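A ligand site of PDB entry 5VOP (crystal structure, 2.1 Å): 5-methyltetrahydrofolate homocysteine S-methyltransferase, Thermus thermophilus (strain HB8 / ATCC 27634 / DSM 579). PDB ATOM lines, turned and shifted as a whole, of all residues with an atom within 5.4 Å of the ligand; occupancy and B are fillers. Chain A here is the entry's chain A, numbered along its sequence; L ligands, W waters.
The side-chain carboxylate (OD2) of Asp 179 lies within hydrogen-bond range of a nitrogen (N3) of the ligand (2.6 Å). The backbone carbonyl oxygen (O) of Gly 27 lies within hydrogen-bond range of a nitrogen (N7) of the ligand (2.9 Å). A nitrogen (N5) of the ligand is in hydrogen-bond range of the side-chain carboxylate (OD2) of Asp 91, at 2.9 Å. The side-chain amide oxygen of Asn 221 lies close to an oxygen (O1) of the ligand, 2.9 Å away. The side-chain amide oxygen of Asn 112 sits at hydrogen-bond distance from a nitrogen (N2) of the ligand (2.9 Å). NH1 of Arg 231 lies within salt-bridge range of O5 of the ligand (3.1 Å). N of Lys 29 lies within hydrogen-bond range of O4 of the ligand.
The side-chain carboxylate (OD2) of Asp 91 sits at hydrogen-bond distance from the side-chain amide nitrogen (ND2) of Asn 112 (3.4 Å). The side-chain carboxylate (OD2) of Asp 91 sits close to the side-chain carboxylate (OD2) of Asp 59. OD1 of Asn 221 sits close to O of Gly 218 (3.0 Å). The side-chain amide nitrogen (ND2) of Asn 112 is in hydrogen-bond range of the side-chain carboxylate (OD1) of Asp 59, 3.3 Å away. N of Arg 30 lies close to OG of Ser 28. The backbone NH of Ile 251 sits at hydrogen-bond distance from the backbone carbonyl oxygen of Leu 217 (2.9 Å). OE1 of Glu 21 lies within hydrogen-bond range of OG of Ser 220 (2.6 Å). The side-chain amide oxygen (OD1) of Asn 24 sits at hydrogen-bond distance from the side-chain hydroxyl (OG1) of Thr 26.
Glu 21 touches the ligand (OE2 to C10, 3.7 Å). ND2 of Asn 24 touches C11 of the ligand, at 3.9 Å. Ser 28 touches the ligand (CA to O4, 3.5 Å). Val 138 touches the ligand (CG1 to N2, 3.8 Å). Leu 140 touches the ligand (CD2 to N2, 3.95 Å). Gly 218 touches the ligand (CA to O1, 3.5 Å). Ser 220 touches the ligand (CB to C14, 3.8 Å). Phe 224 touches the ligand (CE1 to O5, 3.5 Å). CD1 of Ile 251 touches N1 of the ligand (3.5 Å). Within 4 Å of the ligand: Glu 21, Asn 24, Gly 27, Ser 28, Lys 29, Asp 91, Asn 112, Val 138, Leu 140, Asp 179, Gly 218, Ser 220, Asn 221, Phe 224, Arg 231 and Ile 251.
Water W7 lies within hydrogen-bond range of O3 of the ligand, N of Arg 30 and N of Lys 29. Water W6 lies within hydrogen-bond range of the side-chain carboxylate (OD1) of Asp 179, an oxygen (O1) of the ligand, the side-chain hydroxyl (OG1) of Thr 182 and the backbone NH (N) of Gly 218. Water W4 bridges O1 of the ligand (2.8 Å) and N of Thr 182 (2.9 Å). Water W5 lies within hydrogen-bond range of OD2 of Asp 59 (2.7 Å), ND2 of Asn 24 (2.8 Å), O of Glu 21 (2.8 Å) and N6 of the ligand (2.9 Å). Water W8 lies within hydrogen-bond range of the side-chain carboxylate (OE2) of Glu 21 (2.6 Å), an oxygen (O2) of the ligand (3.0 Å) and the side-chain hydroxyl (OG) of Ser 220 (3.4 Å). Water W3 bridges the side-chain carboxylate of Asp 91 (2.8 Å) and a nitrogen (N5) of the ligand (3.3 Å).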
ATOM      1  N   GLU A  21      -7.035  -8.197 -15.889  1.00  0.00           N
ATOM      2  CA  GLU A  21      -5.666  -8.306 -15.360  1.00  0.00           C
ATOM      3  C   GLU A  21      -5.193  -9.736 -15.128  1.00  0.00           C
ATOM      4  O   GLU A  21      -4.017  -9.943 -14.821  1.00  0.00           O
ATOM      5  CB  GLU A  21      -5.558  -7.528 -14.041  1.00  0.00           C
ATOM      6  CG  GLU A  21      -6.119  -8.233 -12.814  1.00  0.00           C
ATOM      7  CD  GLU A  21      -6.098  -7.382 -11.546  1.00  0.00           C
ATOM      8  OE1 GLU A  21      -5.857  -6.158 -11.630  1.00  0.00           O
ATOM      9  OE2 GLU A  21      -6.337  -7.941 -10.450  1.00  0.00           O
ATOM     10  N   ASN A  24      -1.899 -13.417 -15.797  1.00  0.00           N
ATOM     11  CA  ASN A  24      -0.713 -12.803 -15.279  1.00  0.00           C
ATOM     12  C   ASN A  24      -0.067 -13.778 -14.292  1.00  0.00           C
ATOM     13  O   ASN A  24      -0.595 -14.016 -13.201  1.00  0.00           O
ATOM     14  CB  ASN A  24      -1.051 -11.478 -14.604  1.00  0.00           C
ATOM     15  CG  ASN A  24       0.173 -10.683 -14.205  1.00  0.00           C
ATOM     16  OD1 ASN A  24       1.148 -11.251 -13.705  1.00  0.00           O
ATOM     17  ND2 ASN A  24       0.159  -9.389 -14.453  1.00  0.00           N
ATOM     18  N   THR A  26       2.732 -13.886 -12.372  1.00  0.00           N
ATOM     19  CA  THR A  26       3.039 -13.373 -11.030  1.00  0.00           C
ATOM     20  C   THR A  26       1.808 -12.836 -10.313  1.00  0.00           C
ATOM     21  O   THR A  26       1.710 -12.945  -9.098  1.00  0.00           O
ATOM     22  CB  THR A  26       4.117 -12.262 -11.029  1.00  0.00           C
ATOM     23  OG1 THR A  26       3.678 -11.176 -11.841  1.00  0.00           O
ATOM     24  CG2 THR A  26       5.442 -12.782 -11.548  1.00  0.00           C
ATOM     25  N   GLY A  27       0.868 -12.253 -11.051  1.00  0.00           N
ATOM     26  CA  GLY A  27      -0.360 -11.681 -10.461  1.00  0.00           C
ATOM     27  C   GLY A  27      -1.511 -12.635 -10.161  1.00  0.00           C
ATOM     28  O   GLY A  27      -2.513 -12.199  -9.605  1.00  0.00           O
ATOM     29  N   SER A  28      -1.400 -13.919 -10.542  1.00  0.00           N
ATOM     30  CA  SER A  28      -2.531 -14.888 -10.375  1.00  0.00           C
ATOM     31  C   SER A  28      -2.054 -16.310 -10.243  1.00  0.00           C
ATOM     32  O   SER A  28      -1.555 -16.872 -11.218  1.00  0.00           O
ATOM     33  CB  SER A  28      -3.474 -14.804 -11.570  1.00  0.00           C
ATOM     34  OG  SER A  28      -4.375 -15.909 -11.610  1.00  0.00           O
ATOM     35  N   LYS A  29      -2.226 -16.908  -9.074  1.00  0.00           N
ATOM     36  CA  LYS A  29      -1.834 -18.315  -8.858  1.00  0.00           C
ATOM     37  C   LYS A  29      -2.582 -19.255  -9.832  1.00  0.00           C
ATOM     38  O   LYS A  29      -2.014 -20.212 -10.371  1.00  0.00           O
ATOM     39  CB  LYS A  29      -2.099 -18.745  -7.398  1.00  0.00           C
ATOM     40  CG  LYS A  29      -1.162 -19.852  -6.926  1.00  0.00           C
ATOM     41  CD  LYS A  29      -1.728 -20.762  -5.843  1.00  0.00           C
ATOM     42  CE  LYS A  29      -0.612 -21.608  -5.257  1.00  0.00           C
ATOM     43  NZ  LYS A  29      -1.044 -22.698  -4.329  1.00  0.00           N
ATOM     44  N   ARG A  30      -3.858 -18.955 -10.045  1.00  0.00           N
ATOM     45  CA  ARG A  30      -4.737 -19.763 -10.882  1.00  0.00           C
ATOM     46  C   ARG A  30      -4.185 -19.852 -12.306  1.00  0.00           C
ATOM     47  O   ARG A  30      -3.986 -20.935 -12.849  1.00  0.00           O
ATOM     48  CB  ARG A  30      -6.142 -19.152 -10.868  1.00  0.00           C
ATOM     49  CG  ARG A  30      -7.256 -20.060 -11.331  1.00  0.00           C
ATOM     50  CD  ARG A  30      -8.630 -19.361 -11.259  1.00  0.00           C
ATOM     51  NE  ARG A  30      -9.460 -19.734 -12.399  1.00  0.00           N
ATOM     52  CZ  ARG A  30     -10.615 -19.182 -12.761  1.00  0.00           C
ATOM     53  NH1 ARG A  30     -11.168 -18.181 -12.061  1.00  0.00           N
ATOM     54  NH2 ARG A  30     -11.231 -19.640 -13.847  1.00  0.00           N
ATOM     55  N   ASP A  59      -4.948  -8.354 -20.551  1.00  0.00           N
ATOM     56  CA  ASP A  59      -3.529  -8.198 -20.300  1.00  0.00           C
ATOM     57  C   ASP A  59      -2.940  -9.603 -20.192  1.00  0.00           C
ATOM     58  O   ASP A  59      -3.533 -10.473 -19.555  1.00  0.00           O
ATOM     59  CB  ASP A  59      -3.289  -7.425 -19.017  1.00  0.00           C
ATOM     60  CG  ASP A  59      -1.860  -6.980 -18.862  1.00  0.00           C
ATOM     61  OD1 ASP A  59      -1.381  -6.257 -19.771  1.00  0.00           O
ATOM     62  OD2 ASP A  59      -1.227  -7.340 -17.841  1.00  0.00           O
ATOM     63  N   ASP A  91       1.992  -7.875 -22.147  1.00  0.00           N
ATOM     64  CA  ASP A  91       2.586  -7.297 -20.953  1.00  0.00           C
ATOM     65  C   ASP A  91       3.951  -7.965 -20.777  1.00  0.00           C
ATOM     66  O   ASP A  91       4.036  -9.081 -20.299  1.00  0.00           O
ATOM     67  CB  ASP A  91       1.658  -7.576 -19.765  1.00  0.00           C
ATOM     68  CG  ASP A  91       2.064  -6.861 -18.481  1.00  0.00           C
ATOM     69  OD1 ASP A  91       3.247  -6.506 -18.310  1.00  0.00           O
ATOM     70  OD2 ASP A  91       1.173  -6.688 -17.606  1.00  0.00           O
ATOM     71  N   ASN A 112       2.348  -3.320 -23.887  1.00  0.00           N
ATOM     72  CA  ASN A 112       2.534  -2.857 -22.527  1.00  0.00           C
ATOM     73  C   ASN A 112       3.905  -3.329 -22.024  1.00  0.00           C
ATOM     74  O   ASN A 112       4.007  -4.421 -21.479  1.00  0.00           O
ATOM     75  CB  ASN A 112       1.386  -3.420 -21.686  1.00  0.00           C
ATOM     76  CG  ASN A 112       1.469  -3.023 -20.227  1.00  0.00           C
ATOM     77  OD1 ASN A 112       2.112  -2.033 -19.890  1.00  0.00           O
ATOM     78  ND2 ASN A 112       0.833  -3.797 -19.367  1.00  0.00           N
ATOM     79  N   SER A 113       4.977  -2.555 -22.157  1.00  0.00           N
ATOM     80  CA  SER A 113       4.976  -1.142 -22.476  1.00  0.00           C
ATOM     81  C   SER A 113       6.363  -0.675 -22.905  1.00  0.00           C
ATOM     82  O   SER A 113       7.318  -1.430 -22.864  1.00  0.00           O
ATOM     83  CB  SER A 113       4.596  -0.377 -21.221  1.00  0.00           C
ATOM     84  OG  SER A 113       5.501  -0.732 -20.196  1.00  0.00           O
ATOM     85  N   VAL A 138       1.312   1.444 -24.716  1.00  0.00           N
ATOM     86  CA  VAL A 138       1.323   1.942 -23.352  1.00  0.00           C
ATOM     87  C   VAL A 138       2.725   2.490 -23.113  1.00  0.00           C
ATOM     88  O   VAL A 138       3.725   1.804 -23.423  1.00  0.00           O
ATOM     89  CB  VAL A 138       1.069   0.814 -22.326  1.00  0.00           C
ATOM     90  CG1 VAL A 138       1.208   1.311 -20.895  1.00  0.00           C
ATOM     91  CG2 VAL A 138      -0.297   0.192 -22.572  1.00  0.00           C
ATOM     92  N   LEU A 140       5.096   4.123 -19.903  1.00  0.00           N
ATOM     93  CA  LEU A 140       5.148   4.337 -18.456  1.00  0.00           C
ATOM     94  C   LEU A 140       5.943   5.587 -18.151  1.00  0.00           C
ATOM     95  O   LEU A 140       6.971   5.829 -18.782  1.00  0.00           O
ATOM     96  CB  LEU A 140       5.846   3.185 -17.724  1.00  0.00           C
ATOM     97  CG  LEU A 140       5.404   1.744 -17.964  1.00  0.00           C
ATOM     98  CD1 LEU A 140       6.218   0.773 -17.077  1.00  0.00           C
ATOM     99  CD2 LEU A 140       3.918   1.608 -17.699  1.00  0.00           C
ATOM    100  N   ASP A 179       0.744   5.739 -18.923  1.00  0.00           N
ATOM    101  CA  ASP A 179       0.622   5.137 -17.625  1.00  0.00           C
ATOM    102  C   ASP A 179       1.461   5.971 -16.666  1.00  0.00           C
ATOM    103  O   ASP A 179       2.701   5.885 -16.639  1.00  0.00           O
ATOM    104  CB  ASP A 179       1.092   3.690 -17.641  1.00  0.00           C
ATOM    105  CG  ASP A 179       0.840   2.965 -16.317  1.00  0.00           C
ATOM    106  OD1 ASP A 179       0.593   3.616 -15.267  1.00  0.00           O
ATOM    107  OD2 ASP A 179       0.913   1.720 -16.309  1.00  0.00           O
ATOM    108  N   THR A 182       0.681   3.607 -10.781  1.00  0.00           N
ATOM    109  CA  THR A 182      -0.123   3.366  -9.582  1.00  0.00           C
ATOM    110  C   THR A 182       0.747   2.719  -8.515  1.00  0.00           C
ATOM    111  O   THR A 182       1.188   1.597  -8.688  1.00  0.00           O
ATOM    112  CB  THR A 182      -1.275   2.420  -9.934  1.00  0.00           C
ATOM    113  OG1 THR A 182      -1.956   2.954 -11.066  1.00  0.00           O
ATOM    114  CG2 THR A 182      -2.254   2.284  -8.801  1.00  0.00           C
ATOM    115  N   VAL A 216      -3.842   5.010 -19.033  1.00  0.00           N
ATOM    116  CA  VAL A 216      -4.124   3.699 -18.447  1.00  0.00           C
ATOM    117  C   VAL A 216      -3.505   3.595 -17.061  1.00  0.00           C
ATOM    118  O   VAL A 216      -2.465   4.191 -16.798  1.00  0.00           O
ATOM    119  CB  VAL A 216      -3.615   2.541 -19.351  1.00  0.00           C
ATOM    120  CG1 VAL A 216      -2.100   2.534 -19.420  1.00  0.00           C
ATOM    121  CG2 VAL A 216      -4.179   1.196 -18.897  1.00  0.00           C
ATOM    122  N   LEU A 217      -4.166   2.877 -16.175  1.00  0.00           N
ATOM    123  CA  LEU A 217      -3.601   2.575 -14.867  1.00  0.00           C
ATOM    124  C   LEU A 217      -3.827   1.128 -14.531  1.00  0.00           C
ATOM    125  O   LEU A 217      -4.892   0.567 -14.862  1.00  0.00           O
ATOM    126  CB  LEU A 217      -4.239   3.445 -13.770  1.00  0.00           C
ATOM    127  CG  LEU A 217      -3.905   4.940 -13.800  1.00  0.00           C
ATOM    128  CD1 LEU A 217      -4.740   5.660 -12.740  1.00  0.00           C
ATOM    129  CD2 LEU A 217      -2.418   5.182 -13.578  1.00  0.00           C
ATOM    130  N   GLY A 218      -2.828   0.533 -13.878  1.00  0.00           N
ATOM    131  CA  GLY A 218      -2.966  -0.767 -13.222  1.00  0.00           C
ATOM    132  C   GLY A 218      -3.560  -0.527 -11.861  1.00  0.00           C
ATOM    133  O   GLY A 218      -2.855  -0.461 -10.846  1.00  0.00           O
ATOM    134  N   SER A 220      -5.306  -2.034  -9.549  1.00  0.00           N
ATOM    135  CA  SER A 220      -5.213  -2.919  -8.392  1.00  0.00           C
ATOM    136  C   SER A 220      -4.001  -2.643  -7.505  1.00  0.00           C
ATOM    137  O   SER A 220      -4.081  -2.865  -6.306  1.00  0.00           O
ATOM    138  CB  SER A 220      -5.216  -4.387  -8.816  1.00  0.00           C
ATOM    139  OG  SER A 220      -6.407  -4.693  -9.531  1.00  0.00           O
ATOM    140  N   ASN A 221      -2.900  -2.134  -8.085  1.00  0.00           N
ATOM    141  CA  ASN A 221      -1.684  -1.874  -7.323  1.00  0.00           C
ATOM    142  C   ASN A 221      -1.917  -0.903  -6.170  1.00  0.00           C
ATOM    143  O   ASN A 221      -1.170  -0.944  -5.176  1.00  0.00           O
ATOM    144  CB  ASN A 221      -0.559  -1.302  -8.206  1.00  0.00           C
ATOM    145  CG  ASN A 221      -0.220  -2.194  -9.405  1.00  0.00           C
ATOM    146  OD1 ASN A 221      -0.200  -1.738 -10.555  1.00  0.00           O
ATOM    147  ND2 ASN A 221       0.032  -3.446  -9.142  1.00  0.00           N
ATOM    148  N   PHE A 224      -2.571  -2.886  -2.758  1.00  0.00           N
ATOM    149  CA  PHE A 224      -1.822  -4.092  -2.416  1.00  0.00           C
ATOM    150  C   PHE A 224      -1.500  -4.123  -0.923  1.00  0.00           C
ATOM    151  O   PHE A 224      -1.014  -3.131  -0.391  1.00  0.00           O
ATOM    152  CB  PHE A 224      -0.533  -4.235  -3.237  1.00  0.00           C
ATOM    153  CG  PHE A 224       0.095  -5.582  -3.106  1.00  0.00           C
ATOM    154  CD1 PHE A 224      -0.320  -6.644  -3.905  1.00  0.00           C
ATOM    155  CD2 PHE A 224       1.057  -5.822  -2.107  1.00  0.00           C
ATOM    156  CE1 PHE A 224       0.242  -7.906  -3.737  1.00  0.00           C
ATOM    157  CE2 PHE A 224       1.612  -7.076  -1.939  1.00  0.00           C
ATOM    158  CZ  PHE A 224       1.201  -8.121  -2.755  1.00  0.00           C
ATOM    159  N   ARG A 231      -9.514  -3.924  -0.525  1.00  0.00           N
ATOM    160  CA  ARG A 231      -8.933  -3.733  -1.831  1.00  0.00           C
ATOM    161  C   ARG A 231      -9.988  -3.425  -2.892  1.00  0.00           C
ATOM    162  O   ARG A 231      -9.790  -2.525  -3.685  1.00  0.00           O
ATOM    163  CB  ARG A 231      -8.103  -4.974  -2.269  1.00  0.00           C
ATOM    164  CG  ARG A 231      -6.865  -5.236  -1.403  1.00  0.00           C
ATOM    165  CD  ARG A 231      -5.850  -6.193  -2.039  1.00  0.00           C
ATOM    166  NE  ARG A 231      -5.266  -5.588  -3.239  1.00  0.00           N
ATOM    167  CZ  ARG A 231      -4.499  -6.217  -4.120  1.00  0.00           C
ATOM    168  NH1 ARG A 231      -4.161  -7.483  -3.940  1.00  0.00           N
ATOM    169  NH2 ARG A 231      -4.040  -5.566  -5.185  1.00  0.00           N
ATOM    170  N   ILE A 251      -6.438  -1.409 -16.301  1.00  0.00           N
ATOM    171  CA  ILE A 251      -6.082  -2.806 -16.079  1.00  0.00           C
ATOM    172  C   ILE A 251      -6.672  -3.152 -14.707  1.00  0.00           C
ATOM    173  O   ILE A 251      -6.253  -2.606 -13.703  1.00  0.00           O
ATOM    174  CB  ILE A 251      -4.554  -3.037 -16.150  1.00  0.00           C
ATOM    175  CG1 ILE A 251      -4.029  -2.757 -17.571  1.00  0.00           C
ATOM    176  CG2 ILE A 251      -4.178  -4.466 -15.747  1.00  0.00           C
ATOM    177  CD1 ILE A 251      -2.540  -2.421 -17.610  1.00  0.00           C
HETATM  178  N1  LIG L   1       0.844  -2.709 -16.584  1.00  0.00           N
HETATM  179  C1  LIG L   1       0.726  -1.362 -16.540  1.00  0.00           C
HETATM  180  N2  LIG L   1       0.699  -0.682 -17.712  1.00  0.00           N
HETATM  181  N3  LIG L   1       0.629  -0.657 -15.371  1.00  0.00           N
HETATM  182  C2  LIG L   1       0.652  -1.250 -14.156  1.00  0.00           C
HETATM  183  O1  LIG L   1       0.559  -0.561 -13.111  1.00  0.00           O
HETATM  184  C3  LIG L   1       0.773  -2.729 -14.149  1.00  0.00           C
HETATM  185  N4  LIG L   1       0.891  -3.564 -13.041  1.00  0.00           N
HETATM  186  C4  LIG L   1       0.229  -4.875 -13.043  1.00  0.00           C
HETATM  187  C5  LIG L   1       0.991  -5.573 -14.200  1.00  0.00           C
HETATM  188  N5  LIG L   1       1.003  -4.791 -15.443  1.00  0.00           N
HETATM  189  C6  LIG L   1       0.891  -3.436 -15.448  1.00  0.00           C
HETATM  190  C7  LIG L   1      -1.288  -4.838 -13.327  1.00  0.00           C
HETATM  191  N6  LIG L   1      -1.788  -6.206 -13.154  1.00  0.00           N
HETATM  192  C8  LIG L   1       1.945  -3.268 -12.069  1.00  0.00           C
HETATM  193  C9  LIG L   1      -2.644  -8.022  -9.435  1.00  0.00           C
HETATM  194  C10 LIG L   1      -2.730  -8.735 -10.639  1.00  0.00           C
HETATM  195  C11 LIG L   1      -2.444  -8.130 -11.864  1.00  0.00           C
HETATM  196  C12 LIG L   1      -2.070  -6.769 -11.931  1.00  0.00           C
HETATM  197  C13 LIG L   1      -1.979  -6.065 -10.719  1.00  0.00           C
HETATM  198  C14 LIG L   1      -2.264  -6.669  -9.502  1.00  0.00           C
HETATM  199  C15 LIG L   1      -2.930  -8.621  -8.076  1.00  0.00           C
HETATM  200  O2  LIG L   1      -3.071  -7.823  -7.142  1.00  0.00           O
HETATM  201  N7  LIG L   1      -3.001  -9.958  -7.876  1.00  0.00           N
HETATM  202  C16 LIG L   1      -3.262 -10.572  -6.567  1.00  0.00           C
HETATM  203  C17 LIG L   1      -3.339 -12.099  -6.561  1.00  0.00           C
HETATM  204  C18 LIG L   1      -4.613 -12.719  -7.121  1.00  0.00           C
HETATM  205  C19 LIG L   1      -4.595 -14.220  -6.844  1.00  0.00           C
HETATM  206  O3  LIG L   1      -5.638 -14.762  -6.436  1.00  0.00           O
HETATM  207  O4  LIG L   1      -3.555 -14.879  -7.033  1.00  0.00           O
HETATM  208  C20 LIG L   1      -2.157 -10.286  -5.600  1.00  0.00           C
HETATM  209  O5  LIG L   1      -2.477 -10.056  -4.410  1.00  0.00           O
HETATM  210  O6  LIG L   1      -0.979 -10.321  -6.021  1.00  0.00           O
HETATM  211  O   HOH W   1       2.891  -8.330 -13.929  1.00  0.00           O
HETATM  212  O   HOH W   2       3.776  -1.860 -15.599  1.00  0.00           O
HETATM  213  O   HOH W   3       3.780  -6.481 -15.538  1.00  0.00           O
HETATM  214  O   HOH W   4       2.135   1.285 -11.730  1.00  0.00           O
HETATM  215  O   HOH W   5      -2.064  -8.080 -15.409  1.00  0.00           O
HETATM  216  O   HOH W   6      -0.423   2.033 -13.295  1.00  0.00           O
HETATM  217  O   HOH W   7      -5.555 -16.700  -8.229  1.00  0.00           O
HETATM  218  O   HOH W   8      -5.933  -7.644  -7.947  1.00  0.00           O
